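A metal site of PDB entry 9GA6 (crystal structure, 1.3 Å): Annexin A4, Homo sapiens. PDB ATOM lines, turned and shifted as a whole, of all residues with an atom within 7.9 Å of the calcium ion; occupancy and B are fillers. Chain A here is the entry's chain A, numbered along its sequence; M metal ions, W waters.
OE1 of Glu 71 sits close to OG1 of Thr 32, at 2.7 Å.
Four residues have an atom within 4 Å of the calcium ion: Met 27, Gly 29, Gly 31 and Glu 71.
O of Met 27 is bound to the calcium ion, at 2.3 Å. O of Gly 29 binds the calcium ion, 2.3 Å away. The calcium ion is bound by water W1 (2.4 Å). The calcium ion is bound by water W2 (2.4 Å). O of Gly 31 binds the calcium ion. The calcium ion is bound by the side-chain carboxylate (OE2) of Glu 71 (2.5 Å). OE1 of Glu 71 is bound to the calcium ion (2.5 Å).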
ATOM      1  N   ARG A  24     -14.328  15.925  -7.609  1.00  0.00           N
ATOM      2  CA  ARG A  24     -13.372  15.337  -8.541  1.00  0.00           C
ATOM      3  C   ARG A  24     -12.585  16.422  -9.262  1.00  0.00           C
ATOM      4  O   ARG A  24     -11.367  16.290  -9.362  1.00  0.00           O
ATOM      5  CB  ARG A  24     -14.055  14.328  -9.479  1.00  0.00           C
ATOM      6  CG  ARG A  24     -13.195  13.806 -10.622  1.00  0.00           C
ATOM      7  CD  ARG A  24     -12.018  13.041 -10.120  1.00  0.00           C
ATOM      8  NE  ARG A  24     -11.348  12.379 -11.240  1.00  0.00           N
ATOM      9  CZ  ARG A  24     -10.067  12.079 -11.296  1.00  0.00           C
ATOM     10  NH1 ARG A  24      -9.267  12.218 -10.269  1.00  0.00           N
ATOM     11  NH2 ARG A  24      -9.639  11.542 -12.440  1.00  0.00           N
ATOM     12  N   LYS A  25     -13.266  17.420  -9.805  1.00  0.00           N
ATOM     13  CA  LYS A  25     -12.575  18.482 -10.519  1.00  0.00           C
ATOM     14  C   LYS A  25     -11.591  19.198  -9.615  1.00  0.00           C
ATOM     15  O   LYS A  25     -10.484  19.527 -10.059  1.00  0.00           O
ATOM     16  CB  LYS A  25     -13.561  19.527 -11.051  1.00  0.00           C
ATOM     17  CG  LYS A  25     -14.443  19.024 -12.220  1.00  0.00           C
ATOM     18  CD  LYS A  25     -13.741  19.101 -13.562  1.00  0.00           C
ATOM     19  CE  LYS A  25     -14.746  18.829 -14.644  1.00  0.00           C
ATOM     20  NZ  LYS A  25     -14.102  18.990 -15.947  1.00  0.00           N
ATOM     21  N   ALA A  26     -11.895  19.333  -8.318  1.00  0.00           N
ATOM     22  CA  ALA A  26     -11.003  20.001  -7.381  1.00  0.00           C
ATOM     23  C   ALA A  26      -9.702  19.212  -7.191  1.00  0.00           C
ATOM     24  O   ALA A  26      -8.664  19.824  -6.880  1.00  0.00           O
ATOM     25  CB  ALA A  26     -11.698  20.190  -6.046  1.00  0.00           C
ATOM     26  N   MET A  27      -9.719  17.879  -7.304  1.00  0.00           N
ATOM     27  CA  MET A  27      -8.597  17.015  -7.016  1.00  0.00           C
ATOM     28  C   MET A  27      -7.869  16.524  -8.284  1.00  0.00           C
ATOM     29  O   MET A  27      -6.665  16.276  -8.198  1.00  0.00           O
ATOM     30  CB  MET A  27      -9.020  15.837  -6.149  1.00  0.00           C
ATOM     31  CG  MET A  27      -9.455  16.254  -4.780  1.00  0.00           C
ATOM     32  SD  MET A  27      -9.932  14.928  -3.660  1.00  0.00           S
ATOM     33  CE  MET A  27     -11.576  14.637  -4.307  1.00  0.00           C
ATOM     34  N   LYS A  28      -8.578  16.374  -9.401  1.00  0.00           N
ATOM     35  CA  LYS A  28      -7.948  15.817 -10.606  1.00  0.00           C
ATOM     36  C   LYS A  28      -6.771  16.679 -11.043  1.00  0.00           C
ATOM     37  O   LYS A  28      -6.885  17.876 -11.163  1.00  0.00           O
ATOM     38  CB  LYS A  28      -8.994  15.699 -11.707  1.00  0.00           C
ATOM     39  CG  LYS A  28      -8.459  15.046 -12.954  1.00  0.00           C
ATOM     40  CD  LYS A  28      -9.503  14.752 -13.990  1.00  0.00           C
ATOM     41  CE  LYS A  28      -8.902  13.990 -15.137  1.00  0.00           C
ATOM     42  NZ  LYS A  28      -9.864  13.903 -16.221  1.00  0.00           N
ATOM     43  N   GLY A  29      -5.670  16.013 -11.386  1.00  0.00           N
ATOM     44  CA  GLY A  29      -4.518  16.723 -11.925  1.00  0.00           C
ATOM     45  C   GLY A  29      -3.586  17.182 -10.832  1.00  0.00           C
ATOM     46  O   GLY A  29      -3.848  17.077  -9.637  1.00  0.00           O
ATOM     47  N   LEU A  30      -2.422  17.735 -11.224  1.00  0.00           N
ATOM     48  CA  LEU A  30      -1.489  18.238 -10.239  1.00  0.00           C
ATOM     49  C   LEU A  30      -2.163  19.275  -9.348  1.00  0.00           C
ATOM     50  O   LEU A  30      -2.906  20.136  -9.800  1.00  0.00           O
ATOM     51  CB  LEU A  30      -0.287  18.854 -10.970  1.00  0.00           C
ATOM     52  CG  LEU A  30       0.857  19.366 -10.075  1.00  0.00           C
ATOM     53  CD1 LEU A  30       1.419  18.382  -9.079  1.00  0.00           C
ATOM     54  CD2 LEU A  30       1.980  19.911 -10.951  1.00  0.00           C
ATOM     55  N   GLY A  31      -1.910  19.111  -8.062  1.00  0.00           N
ATOM     56  CA  GLY A  31      -2.405  20.016  -7.044  1.00  0.00           C
ATOM     57  C   GLY A  31      -3.868  19.788  -6.687  1.00  0.00           C
ATOM     58  O   GLY A  31      -4.437  18.791  -7.103  1.00  0.00           O
ATOM     59  N   THR A  32      -4.426  20.715  -5.931  1.00  0.00           N
ATOM     60  CA  THR A  32      -5.763  20.590  -5.373  1.00  0.00           C
ATOM     61  C   THR A  32      -6.371  21.969  -5.270  1.00  0.00           C
ATOM     62  O   THR A  32      -5.700  22.972  -4.944  1.00  0.00           O
ATOM     63  CB  THR A  32      -5.616  20.025  -3.942  1.00  0.00           C
ATOM     64  OG1 THR A  32      -4.769  18.901  -3.964  1.00  0.00           O
ATOM     65  CG2 THR A  32      -6.945  19.638  -3.328  1.00  0.00           C
ATOM     66  N   ASP A  33      -7.691  22.064  -5.440  1.00  0.00           N
ATOM     67  CA  ASP A  33      -8.463  23.243  -5.110  1.00  0.00           C
ATOM     68  C   ASP A  33      -9.110  23.027  -3.731  1.00  0.00           C
ATOM     69  O   ASP A  33     -10.265  22.614  -3.654  1.00  0.00           O
ATOM     70  CB  ASP A  33      -9.509  23.573  -6.169  1.00  0.00           C
ATOM     71  CG  ASP A  33     -10.267  24.847  -5.925  1.00  0.00           C
ATOM     72  OD1 ASP A  33     -10.088  25.465  -4.867  1.00  0.00           O
ATOM     73  OD2 ASP A  33     -11.044  25.213  -6.867  1.00  0.00           O
ATOM     74  N   ASP A  67      -9.418   9.493  -2.046  1.00  0.00           N
ATOM     75  CA  ASP A  67      -8.906  10.618  -2.813  1.00  0.00           C
ATOM     76  C   ASP A  67      -8.573  11.785  -1.886  1.00  0.00           C
ATOM     77  O   ASP A  67      -7.529  12.418  -2.034  1.00  0.00           O
ATOM     78  CB  ASP A  67      -9.899  11.044  -3.903  1.00  0.00           C
ATOM     79  CG  ASP A  67      -9.916  10.180  -5.147  1.00  0.00           C
ATOM     80  OD1 ASP A  67      -9.029   9.242  -5.231  1.00  0.00           O
ATOM     81  OD2 ASP A  67     -10.713  10.465  -6.063  1.00  0.00           O
ATOM     82  N   SER A  70      -5.355  11.151  -0.092  1.00  0.00           N
ATOM     83  CA  SER A  70      -4.223  11.265  -1.011  1.00  0.00           C
ATOM     84  C   SER A  70      -3.885  12.721  -1.274  1.00  0.00           C
ATOM     85  O   SER A  70      -2.713  13.074  -1.421  1.00  0.00           O
ATOM     86  CB  SER A  70      -4.495  10.558  -2.315  1.00  0.00           C
ATOM     87  OG  SER A  70      -3.401  10.684  -3.225  1.00  0.00           O
ATOM     88  N   GLU A  71      -4.884  13.570  -1.413  1.00  0.00           N
ATOM     89  CA  GLU A  71      -4.680  14.940  -1.853  1.00  0.00           C
ATOM     90  C   GLU A  71      -4.350  15.902  -0.709  1.00  0.00           C
ATOM     91  O   GLU A  71      -3.655  16.890  -0.931  1.00  0.00           O
ATOM     92  CB  GLU A  71      -5.953  15.431  -2.536  1.00  0.00           C
ATOM     93  CG  GLU A  71      -6.173  14.715  -3.850  1.00  0.00           C
ATOM     94  CD  GLU A  71      -5.574  15.352  -5.079  1.00  0.00           C
ATOM     95  OE1 GLU A  71      -5.498  16.596  -5.179  1.00  0.00           O
ATOM     96  OE2 GLU A  71      -5.238  14.595  -5.991  1.00  0.00           O
HETATM   97 CA    CA M   1      -4.476  16.407  -7.476  1.00  0.00          CA
HETATM   98  O   HOH W   1      -2.422  16.326  -6.329  1.00  0.00           O
HETATM   99  O   HOH W   2      -3.750  14.359  -8.524  1.00  0.00           O
